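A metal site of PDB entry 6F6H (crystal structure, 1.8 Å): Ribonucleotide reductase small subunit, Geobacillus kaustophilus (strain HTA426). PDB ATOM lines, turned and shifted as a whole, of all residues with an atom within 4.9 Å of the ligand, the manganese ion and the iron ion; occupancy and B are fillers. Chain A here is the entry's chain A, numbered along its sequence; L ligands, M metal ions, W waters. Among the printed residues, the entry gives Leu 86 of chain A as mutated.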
ATOM      1  N   LEU A  75      14.292 -33.078  10.233  1.00  0.00           N
ATOM      2  CA  LEU A  75      13.552 -31.837  10.321  1.00  0.00           C
ATOM      3  C   LEU A  75      13.072 -31.593  11.749  1.00  0.00           C
ATOM      4  O   LEU A  75      13.209 -30.469  12.258  1.00  0.00           O
ATOM      5  CB  LEU A  75      12.369 -31.871   9.345  1.00  0.00           C
ATOM      6  CG  LEU A  75      11.800 -30.518   8.888  1.00  0.00           C
ATOM      7  CD1 LEU A  75      12.879 -29.720   8.122  1.00  0.00           C
ATOM      8  CD2 LEU A  75      10.572 -30.702   8.014  1.00  0.00           C
ATOM      9  N   GLY A  78      15.884 -30.498  13.921  1.00  0.00           N
ATOM     10  CA  GLY A  78      16.264 -29.117  13.706  1.00  0.00           C
ATOM     11  C   GLY A  78      15.333 -28.171  14.437  1.00  0.00           C
ATOM     12  O   GLY A  78      15.781 -27.212  15.071  1.00  0.00           O
ATOM     13  N   PHE A  79      14.022 -28.439  14.363  1.00  0.00           N
ATOM     14  CA  PHE A  79      13.069 -27.592  15.075  1.00  0.00           C
ATOM     15  C   PHE A  79      13.218 -27.739  16.578  1.00  0.00           C
ATOM     16  O   PHE A  79      13.226 -26.729  17.299  1.00  0.00           O
ATOM     17  CB  PHE A  79      11.633 -27.922  14.676  1.00  0.00           C
ATOM     18  CG  PHE A  79      11.113 -27.045  13.557  1.00  0.00           C
ATOM     19  CD1 PHE A  79      10.660 -25.761  13.815  1.00  0.00           C
ATOM     20  CD2 PHE A  79      11.096 -27.510  12.254  1.00  0.00           C
ATOM     21  CE1 PHE A  79      10.201 -24.958  12.759  1.00  0.00           C
ATOM     22  CE2 PHE A  79      10.626 -26.722  11.211  1.00  0.00           C
ATOM     23  CZ  PHE A  79      10.195 -25.463  11.466  1.00  0.00           C
ATOM     24  N   GLY A  82      16.022 -25.800  17.841  1.00  0.00           N
ATOM     25  CA  GLY A  82      15.699 -24.397  17.575  1.00  0.00           C
ATOM     26  C   GLY A  82      14.745 -23.794  18.591  1.00  0.00           C
ATOM     27  O   GLY A  82      15.004 -22.724  19.148  1.00  0.00           O
ATOM     28  N   GLU A  83      13.608 -24.455  18.824  1.00  0.00           N
ATOM     29  CA  GLU A  83      12.653 -23.975  19.818  1.00  0.00           C
ATOM     30  C   GLU A  83      13.306 -23.814  21.180  1.00  0.00           C
ATOM     31  O   GLU A  83      13.066 -22.812  21.893  1.00  0.00           O
ATOM     32  CB  GLU A  83      11.459 -24.935  19.956  1.00  0.00           C
ATOM     33  CG  GLU A  83      10.727 -25.293  18.654  1.00  0.00           C
ATOM     34  CD  GLU A  83      10.238 -24.097  17.838  1.00  0.00           C
ATOM     35  OE1 GLU A  83      10.151 -22.967  18.371  1.00  0.00           O
ATOM     36  OE2 GLU A  83       9.890 -24.305  16.656  1.00  0.00           O
ATOM     37  N   LEU A  86      15.723 -20.894  21.204  1.00  0.00           N
ATOM     38  CA  LEU A  86      15.020 -19.627  21.161  1.00  0.00           C
ATOM     39  C   LEU A  86      14.285 -19.338  22.459  1.00  0.00           C
ATOM     40  O   LEU A  86      14.152 -18.173  22.838  1.00  0.00           O
ATOM     41  CB  LEU A  86      14.075 -19.598  19.964  1.00  0.00           C
ATOM     42  CG  LEU A  86      14.729 -18.964  18.725  1.00  0.00           C
ATOM     43  CD1 LEU A  86      15.943 -19.636  18.242  1.00  0.00           C
ATOM     44  CD2 LEU A  86      13.712 -18.954  17.595  1.00  0.00           C
ATOM     45  N   PHE A 112       6.140 -13.452  23.490  1.00  0.00           N
ATOM     46  CA  PHE A 112       7.159 -14.087  22.649  1.00  0.00           C
ATOM     47  C   PHE A 112       7.768 -15.301  23.374  1.00  0.00           C
ATOM     48  O   PHE A 112       7.831 -16.415  22.820  1.00  0.00           O
ATOM     49  CB  PHE A 112       8.213 -13.009  22.308  1.00  0.00           C
ATOM     50  CG  PHE A 112       9.108 -13.318  21.140  1.00  0.00           C
ATOM     51  CD1 PHE A 112       9.556 -12.310  20.326  1.00  0.00           C
ATOM     52  CD2 PHE A 112       9.608 -14.594  20.921  1.00  0.00           C
ATOM     53  CE1 PHE A 112      10.382 -12.578  19.254  1.00  0.00           C
ATOM     54  CE2 PHE A 112      10.447 -14.859  19.864  1.00  0.00           C
ATOM     55  CZ  PHE A 112      10.816 -13.849  19.012  1.00  0.00           C
ATOM     56  N   GLU A 116       7.517 -19.498  22.511  1.00  0.00           N
ATOM     57  CA  GLU A 116       8.611 -20.415  22.222  1.00  0.00           C
ATOM     58  C   GLU A 116       8.614 -21.593  23.199  1.00  0.00           C
ATOM     59  O   GLU A 116       8.923 -22.726  22.806  1.00  0.00           O
ATOM     60  CB  GLU A 116       9.963 -19.661  22.271  1.00  0.00           C
ATOM     61  CG  GLU A 116      10.027 -18.500  21.251  1.00  0.00           C
ATOM     62  CD  GLU A 116      10.076 -18.907  19.785  1.00  0.00           C
ATOM     63  OE1 GLU A 116       9.952 -20.108  19.438  1.00  0.00           O
ATOM     64  OE2 GLU A 116      10.205 -17.990  18.959  1.00  0.00           O
ATOM     65  N   HIS A 119       6.219 -23.931  21.792  1.00  0.00           N
ATOM     66  CA  HIS A 119       6.843 -24.617  20.664  1.00  0.00           C
ATOM     67  C   HIS A 119       7.728 -25.783  21.109  1.00  0.00           C
ATOM     68  O   HIS A 119       7.662 -26.877  20.519  1.00  0.00           O
ATOM     69  CB  HIS A 119       7.638 -23.614  19.851  1.00  0.00           C
ATOM     70  CG  HIS A 119       6.805 -22.505  19.300  1.00  0.00           C
ATOM     71  ND1 HIS A 119       7.286 -21.572  18.400  1.00  0.00           N
ATOM     72  CD2 HIS A 119       5.494 -22.204  19.480  1.00  0.00           C
ATOM     73  CE1 HIS A 119       6.319 -20.717  18.086  1.00  0.00           C
ATOM     74  NE2 HIS A 119       5.222 -21.087  18.725  1.00  0.00           N
ATOM     75  N   TYR A 145      24.624 -26.271  11.135  1.00  0.00           N
ATOM     76  CA  TYR A 145      23.568 -26.082  12.128  1.00  0.00           C
ATOM     77  C   TYR A 145      24.165 -25.642  13.472  1.00  0.00           C
ATOM     78  O   TYR A 145      23.665 -24.719  14.119  1.00  0.00           O
ATOM     79  CB  TYR A 145      22.749 -27.353  12.273  1.00  0.00           C
ATOM     80  CG  TYR A 145      21.583 -27.198  13.180  1.00  0.00           C
ATOM     81  CD1 TYR A 145      20.325 -26.888  12.679  1.00  0.00           C
ATOM     82  CD2 TYR A 145      21.698 -27.401  14.534  1.00  0.00           C
ATOM     83  CE1 TYR A 145      19.249 -26.750  13.508  1.00  0.00           C
ATOM     84  CE2 TYR A 145      20.635 -27.260  15.378  1.00  0.00           C
ATOM     85  CZ  TYR A 145      19.395 -26.953  14.848  1.00  0.00           C
ATOM     86  OH  TYR A 145      18.330 -26.800  15.665  1.00  0.00           O
ATOM     87  N   PHE A 149      23.050 -22.467  15.778  1.00  0.00           N
ATOM     88  CA  PHE A 149      22.232 -22.641  16.975  1.00  0.00           C
ATOM     89  C   PHE A 149      23.023 -22.902  18.261  1.00  0.00           C
ATOM     90  O   PHE A 149      22.569 -22.518  19.350  1.00  0.00           O
ATOM     91  CB  PHE A 149      21.254 -23.788  16.733  1.00  0.00           C
ATOM     92  CG  PHE A 149      20.143 -23.407  15.795  1.00  0.00           C
ATOM     93  CD1 PHE A 149      19.031 -22.758  16.271  1.00  0.00           C
ATOM     94  CD2 PHE A 149      20.242 -23.676  14.440  1.00  0.00           C
ATOM     95  CE1 PHE A 149      18.004 -22.404  15.411  1.00  0.00           C
ATOM     96  CE2 PHE A 149      19.218 -23.311  13.588  1.00  0.00           C
ATOM     97  CZ  PHE A 149      18.103 -22.674  14.070  1.00  0.00           C
ATOM     98  N   VAL A 180      17.134 -17.103  11.874  1.00  0.00           N
ATOM     99  CA  VAL A 180      16.557 -18.330  12.445  1.00  0.00           C
ATOM    100  C   VAL A 180      15.059 -18.372  12.208  1.00  0.00           C
ATOM    101  O   VAL A 180      14.526 -19.371  11.710  1.00  0.00           O
ATOM    102  CB  VAL A 180      16.915 -18.456  13.921  1.00  0.00           C
ATOM    103  CG1 VAL A 180      16.191 -19.617  14.545  1.00  0.00           C
ATOM    104  CG2 VAL A 180      18.472 -18.628  14.069  1.00  0.00           C
ATOM    105  N   GLU A 181      14.338 -17.315  12.587  1.00  0.00           N
ATOM    106  CA  GLU A 181      12.886 -17.299  12.423  1.00  0.00           C
ATOM    107  C   GLU A 181      12.480 -17.013  10.979  1.00  0.00           C
ATOM    108  O   GLU A 181      11.710 -17.774  10.361  1.00  0.00           O
ATOM    109  CB  GLU A 181      12.275 -16.253  13.367  1.00  0.00           C
ATOM    110  CG  GLU A 181      12.270 -16.752  14.802  1.00  0.00           C
ATOM    111  CD  GLU A 181      11.765 -15.791  15.839  1.00  0.00           C
ATOM    112  OE1 GLU A 181      11.983 -14.579  15.684  1.00  0.00           O
ATOM    113  OE2 GLU A 181      11.162 -16.269  16.848  1.00  0.00           O
ATOM    114  N   LEU A 184      14.979 -19.778   8.324  1.00  0.00           N
ATOM    115  CA  LEU A 184      14.939 -21.220   8.555  1.00  0.00           C
ATOM    116  C   LEU A 184      13.555 -21.706   9.022  1.00  0.00           C
ATOM    117  O   LEU A 184      13.012 -22.659   8.459  1.00  0.00           O
ATOM    118  CB  LEU A 184      16.011 -21.628   9.545  1.00  0.00           C
ATOM    119  CG  LEU A 184      17.422 -21.555   9.007  1.00  0.00           C
ATOM    120  CD1 LEU A 184      18.406 -21.821  10.177  1.00  0.00           C
ATOM    121  CD2 LEU A 184      17.620 -22.590   7.918  1.00  0.00           C
ATOM    122  N   ALA A 185      12.962 -21.084  10.051  1.00  0.00           N
ATOM    123  CA  ALA A 185      11.696 -21.634  10.557  1.00  0.00           C
ATOM    124  C   ALA A 185      10.631 -21.571   9.489  1.00  0.00           C
ATOM    125  O   ALA A 185       9.858 -22.521   9.318  1.00  0.00           O
ATOM    126  CB  ALA A 185      11.191 -20.892  11.773  1.00  0.00           C
ATOM    127  N   SER A 187      10.950 -21.653   6.310  1.00  0.00           N
ATOM    128  CA  SER A 187      11.194 -22.629   5.279  1.00  0.00           C
ATOM    129  C   SER A 187      10.924 -24.023   5.802  1.00  0.00           C
ATOM    130  O   SER A 187      10.478 -24.884   5.045  1.00  0.00           O
ATOM    131  CB  SER A 187      12.621 -22.457   4.739  1.00  0.00           C
ATOM    132  OG  SER A 187      12.778 -21.155   4.195  1.00  0.00           O
ATOM    133  N   GLY A 188      11.107 -24.244   7.113  1.00  0.00           N
ATOM    134  CA  GLY A 188      10.687 -25.494   7.734  1.00  0.00           C
ATOM    135  C   GLY A 188       9.182 -25.707   7.690  1.00  0.00           C
ATOM    136  O   GLY A 188       8.712 -26.817   7.408  1.00  0.00           O
ATOM    137  N   TYR A 189       8.404 -24.674   8.044  1.00  0.00           N
ATOM    138  CA  TYR A 189       6.928 -24.802   7.975  1.00  0.00           C
ATOM    139  C   TYR A 189       6.503 -25.186   6.578  1.00  0.00           C
ATOM    140  O   TYR A 189       5.651 -26.061   6.386  1.00  0.00           O
ATOM    141  CB  TYR A 189       6.243 -23.484   8.366  1.00  0.00           C
ATOM    142  CG  TYR A 189       6.608 -22.988   9.732  1.00  0.00           C
ATOM    143  CD1 TYR A 189       6.811 -23.874  10.771  1.00  0.00           C
ATOM    144  CD2 TYR A 189       6.764 -21.622  10.001  1.00  0.00           C
ATOM    145  CE1 TYR A 189       7.179 -23.437  12.023  1.00  0.00           C
ATOM    146  CE2 TYR A 189       7.136 -21.171  11.234  1.00  0.00           C
ATOM    147  CZ  TYR A 189       7.334 -22.090  12.268  1.00  0.00           C
ATOM    148  OH  TYR A 189       7.713 -21.671  13.526  1.00  0.00           O
ATOM    149  N   THR A 191       8.323 -26.628   4.186  1.00  0.00           N
ATOM    150  CA  THR A 191       8.756 -27.988   3.891  1.00  0.00           C
ATOM    151  C   THR A 191       7.822 -29.031   4.510  1.00  0.00           C
ATOM    152  O   THR A 191       7.466 -30.024   3.853  1.00  0.00           O
ATOM    153  CB  THR A 191      10.195 -28.182   4.390  1.00  0.00           C
ATOM    154  OG1 THR A 191      11.080 -27.308   3.664  1.00  0.00           O
ATOM    155  CG2 THR A 191      10.675 -29.602   4.196  1.00  0.00           C
ATOM    156  N   GLU A 216       4.825 -17.232  14.641  1.00  0.00           N
ATOM    157  CA  GLU A 216       6.035 -16.712  13.988  1.00  0.00           C
ATOM    158  C   GLU A 216       5.820 -15.351  13.349  1.00  0.00           C
ATOM    159  O   GLU A 216       6.730 -14.527  13.308  1.00  0.00           O
ATOM    160  CB  GLU A 216       6.521 -17.675  12.915  1.00  0.00           C
ATOM    161  CG  GLU A 216       8.012 -17.702  12.723  1.00  0.00           C
ATOM    162  CD  GLU A 216       8.666 -18.198  13.977  1.00  0.00           C
ATOM    163  OE1 GLU A 216       8.812 -19.418  14.119  1.00  0.00           O
ATOM    164  OE2 GLU A 216       8.986 -17.354  14.836  1.00  0.00           O
ATOM    165  N   HIS A 219       6.696 -12.878  15.872  1.00  0.00           N
ATOM    166  CA  HIS A 219       8.115 -12.892  16.214  1.00  0.00           C
ATOM    167  C   HIS A 219       8.932 -12.149  15.164  1.00  0.00           C
ATOM    168  O   HIS A 219       9.798 -11.326  15.485  1.00  0.00           O
ATOM    169  CB  HIS A 219       8.584 -14.347  16.385  1.00  0.00           C
ATOM    170  CG  HIS A 219       7.807 -15.098  17.414  1.00  0.00           C
ATOM    171  ND1 HIS A 219       8.057 -16.414  17.746  1.00  0.00           N
ATOM    172  CD2 HIS A 219       6.784 -14.698  18.198  1.00  0.00           C
ATOM    173  CE1 HIS A 219       7.227 -16.785  18.713  1.00  0.00           C
ATOM    174  NE2 HIS A 219       6.436 -15.768  18.986  1.00  0.00           N
ATOM    175  N   TYR A 255      23.309 -25.949   5.931  1.00  0.00           N
ATOM    176  CA  TYR A 255      22.400 -26.838   6.640  1.00  0.00           C
ATOM    177  C   TYR A 255      21.316 -27.361   5.701  1.00  0.00           C
ATOM    178  O   TYR A 255      21.016 -28.557   5.684  1.00  0.00           O
ATOM    179  CB  TYR A 255      21.787 -26.124   7.822  1.00  0.00           C
ATOM    180  CG  TYR A 255      20.696 -26.900   8.555  1.00  0.00           C
ATOM    181  CD1 TYR A 255      20.948 -28.117   9.127  1.00  0.00           C
ATOM    182  CD2 TYR A 255      19.454 -26.349   8.731  1.00  0.00           C
ATOM    183  CE1 TYR A 255      20.001 -28.796   9.825  1.00  0.00           C
ATOM    184  CE2 TYR A 255      18.449 -27.055   9.431  1.00  0.00           C
ATOM    185  CZ  TYR A 255      18.736 -28.259   9.971  1.00  0.00           C
ATOM    186  OH  TYR A 255      17.775 -28.943  10.682  1.00  0.00           O
ATOM    187  N   VAL A 256      20.752 -26.469   4.889  1.00  0.00           N
ATOM    188  CA  VAL A 256      19.680 -26.855   3.973  1.00  0.00           C
ATOM    189  C   VAL A 256      20.174 -27.920   2.989  1.00  0.00           C
ATOM    190  O   VAL A 256      19.472 -28.890   2.718  1.00  0.00           O
ATOM    191  CB  VAL A 256      19.142 -25.610   3.248  1.00  0.00           C
ATOM    192  CG1 VAL A 256      18.346 -25.997   2.033  1.00  0.00           C
ATOM    193  CG2 VAL A 256      18.316 -24.742   4.193  1.00  0.00           C
ATOM    194  N   LEU A 259      20.260 -31.271   4.866  1.00  0.00           N
ATOM    195  CA  LEU A 259      18.924 -31.862   4.902  1.00  0.00           C
ATOM    196  C   LEU A 259      18.533 -32.396   3.523  1.00  0.00           C
ATOM    197  O   LEU A 259      17.893 -33.440   3.423  1.00  0.00           O
ATOM    198  CB  LEU A 259      17.893 -30.840   5.347  1.00  0.00           C
ATOM    199  CG  LEU A 259      17.951 -30.423   6.810  1.00  0.00           C
ATOM    200  CD1 LEU A 259      16.965 -29.276   7.008  1.00  0.00           C
ATOM    201  CD2 LEU A 259      17.645 -31.589   7.723  1.00  0.00           C
ATOM    202  N   THR A 260      18.875 -31.664   2.467  1.00  0.00           N
ATOM    203  CA  THR A 260      18.498 -32.072   1.125  1.00  0.00           C
ATOM    204  C   THR A 260      19.159 -33.387   0.741  1.00  0.00           C
ATOM    205  O   THR A 260      18.518 -34.310   0.221  1.00  0.00           O
ATOM    206  CB  THR A 260      18.885 -30.969   0.150  1.00  0.00           C
ATOM    207  OG1 THR A 260      18.001 -29.864   0.331  1.00  0.00           O
ATOM    208  CG2 THR A 260      18.775 -31.448  -1.272  1.00  0.00           C
ATOM    209  N   TYR A 279      13.074 -30.973  -4.186  1.00  0.00           N
ATOM    210  CA  TYR A 279      14.054 -30.361  -3.288  1.00  0.00           C
ATOM    211  C   TYR A 279      14.653 -29.103  -3.883  1.00  0.00           C
ATOM    212  O   TYR A 279      15.036 -28.196  -3.144  1.00  0.00           O
ATOM    213  CB  TYR A 279      15.156 -31.336  -2.943  1.00  0.00           C
ATOM    214  CG  TYR A 279      14.698 -32.429  -2.054  1.00  0.00           C
ATOM    215  CD1 TYR A 279      14.407 -32.183  -0.713  1.00  0.00           C
ATOM    216  CD2 TYR A 279      14.537 -33.730  -2.543  1.00  0.00           C
ATOM    217  CE1 TYR A 279      13.966 -33.190   0.108  1.00  0.00           C
ATOM    218  CE2 TYR A 279      14.103 -34.734  -1.728  1.00  0.00           C
ATOM    219  CZ  TYR A 279      13.810 -34.475  -0.415  1.00  0.00           C
ATOM    220  OH  TYR A 279      13.368 -35.500   0.383  1.00  0.00           O
ATOM    221  N   LEU A 282      12.359 -26.471  -2.763  1.00  0.00           N
ATOM    222  CA  LEU A 282      12.522 -26.099  -1.375  1.00  0.00           C
ATOM    223  C   LEU A 282      13.742 -25.221  -1.187  1.00  0.00           C
ATOM    224  O   LEU A 282      13.677 -24.209  -0.482  1.00  0.00           O
ATOM    225  CB  LEU A 282      12.619 -27.354  -0.498  1.00  0.00           C
ATOM    226  CG  LEU A 282      11.342 -28.195  -0.505  1.00  0.00           C
ATOM    227  CD1 LEU A 282      11.506 -29.478   0.235  1.00  0.00           C
ATOM    228  CD2 LEU A 282      10.135 -27.436   0.054  1.00  0.00           C
ATOM    229  N   VAL A 286      13.975 -21.177   0.334  1.00  0.00           N
ATOM    230  CA  VAL A 286      14.881 -20.676   1.380  1.00  0.00           C
ATOM    231  C   VAL A 286      15.618 -19.435   0.908  1.00  0.00           C
ATOM    232  O   VAL A 286      15.638 -18.408   1.603  1.00  0.00           O
ATOM    233  CB  VAL A 286      15.861 -21.780   1.800  1.00  0.00           C
ATOM    234  CG1 VAL A 286      16.932 -21.222   2.772  1.00  0.00           C
ATOM    235  CG2 VAL A 286      15.107 -22.921   2.447  1.00  0.00           C
HETATM  236  C1  LIG L   1      11.407 -20.542  16.175  1.00  0.00           C
HETATM  237  O1  LIG L   1      11.080 -21.328  17.104  1.00  0.00           O
HETATM  238  O2  LIG L   1      11.001 -19.344  15.931  1.00  0.00           O
HETATM  239  C2  LIG L   1      12.519 -21.044  15.231  1.00  0.00           C
HETATM  240  C3  LIG L   1      12.855 -22.522  15.268  1.00  0.00           C
HETATM  241  C4  LIG L   1      14.100 -22.859  14.412  1.00  0.00           C
HETATM  242  C5  LIG L   1      13.873 -23.939  13.371  1.00  0.00           C
HETATM  243  C6  LIG L   1      15.122 -24.429  12.668  1.00  0.00           C
HETATM  244  C7  LIG L   1      14.904 -25.723  11.879  1.00  0.00           C
HETATM  245  C8  LIG L   1      14.175 -25.526  10.587  1.00  0.00           C
HETATM  246  C9  LIG L   1      14.595 -26.449   9.446  1.00  0.00           C
HETATM  247  C10 LIG L   1      14.863 -25.689   8.141  1.00  0.00           C
HETATM  248  C11 LIG L   1      14.474 -26.472   6.932  1.00  0.00           C
HETATM  249  C12 LIG L   1      14.731 -25.727   5.639  1.00  0.00           C
HETATM  250  C13 LIG L   1      14.299 -26.507   4.387  1.00  0.00           C
HETATM  251  C14 LIG L   1      15.197 -27.668   3.999  1.00  0.00           C
HETATM  252  C15 LIG L   1      14.719 -28.479   2.806  1.00  0.00           C
HETATM  253  C16 LIG L   1      14.911 -29.990   2.949  1.00  0.00           C
HETATM  254 MN    MN M   1       9.416 -21.166  17.686  1.00  0.00          MN
HETATM  255 FE    FE M   2       9.712 -17.771  16.956  1.00  0.00          FE
HETATM  256  O   HOH W   1       8.530 -19.535  16.648  1.00  0.00           O
HETATM  257  O   HOH W   2       8.970 -22.468  15.835  1.00  0.00           O
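The manganese ion is bound by O1 of the ligand (1.8 Å), OE1 of Glu 83 (2.1 Å), OE1 of Glu 116 (2.1 Å), water W1 (2.1 Å), ND1 of His 119 (2.3 Å) and water W2 (2.3 Å).
The manganese ion has six donor atoms within binding distance.
OH of Tyr 189 is in hydrogen-bond range of OE1 of Glu 216 (2.6 Å).
OG1 of Thr 191 sits at hydrogen-bond distance from O of Ser 187.
The backbone carbonyl oxygen of Gly 78 sits at hydrogen-bond distance from the side-chain hydroxyl of Tyr 145 (2.6 Å).
N of Ala 185 lies within hydrogen-bond range of O of Val 180, 2.9 Å away.
N of Gly 82 is in hydrogen-bond range of OH of Tyr 145 (3.3 Å).
O of Val 256 is in hydrogen-bond range of OG1 of Thr 260 (3.0 Å).
CD1 of Leu 75 touches C11 of the ligand (3.8 Å).
C of Gly 78 touches C7 of the ligand, at 3.6 Å.
Phe 79 touches the ligand.
CA of Gly 82 touches C4 of the ligand, at 3.9 Å.
Leu 86 touches the ligand (CD2 to C1, 3.1 Å).
CZ of Phe 149 touches C6 of the ligand (3.7 Å).
Val 180 touches the ligand.
Leu 184 touches the ligand (O to C10, 3.6 Å).
Ala 185 touches the ligand (CB to C2, 3.7 Å).
Ser 187 touches the ligand.
Gly 188 touches the ligand.
Thr 191 touches the ligand (OG1 to C13, 3.4 Å).
Tyr 255 touches the ligand (CE2 to C9, 3.9 Å).
Val 256 touches the ligand (CG2 to C12, 3.99 Å).
Leu 259 touches the ligand.
Hydrophobic or aromatic side chains that line the ligand: Leu 75, Phe 79, Leu 86, Phe 149, Val 180, Ala 185, Tyr 255, Val 256 and Leu 259.
Of the 28 residues printed, 19 come within 4 Å of the ligand.
Of the 28 residues printed, 3 come within 4 Å of the manganese ion.
The iron ion is bound by OE2 of Glu 116, OE2 of Glu 181, water W1, O2 of the ligand, OE2 of Glu 216 and ND1 of His 219.
Of the 28 residues printed, 4 come within 4 Å of the iron ion.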
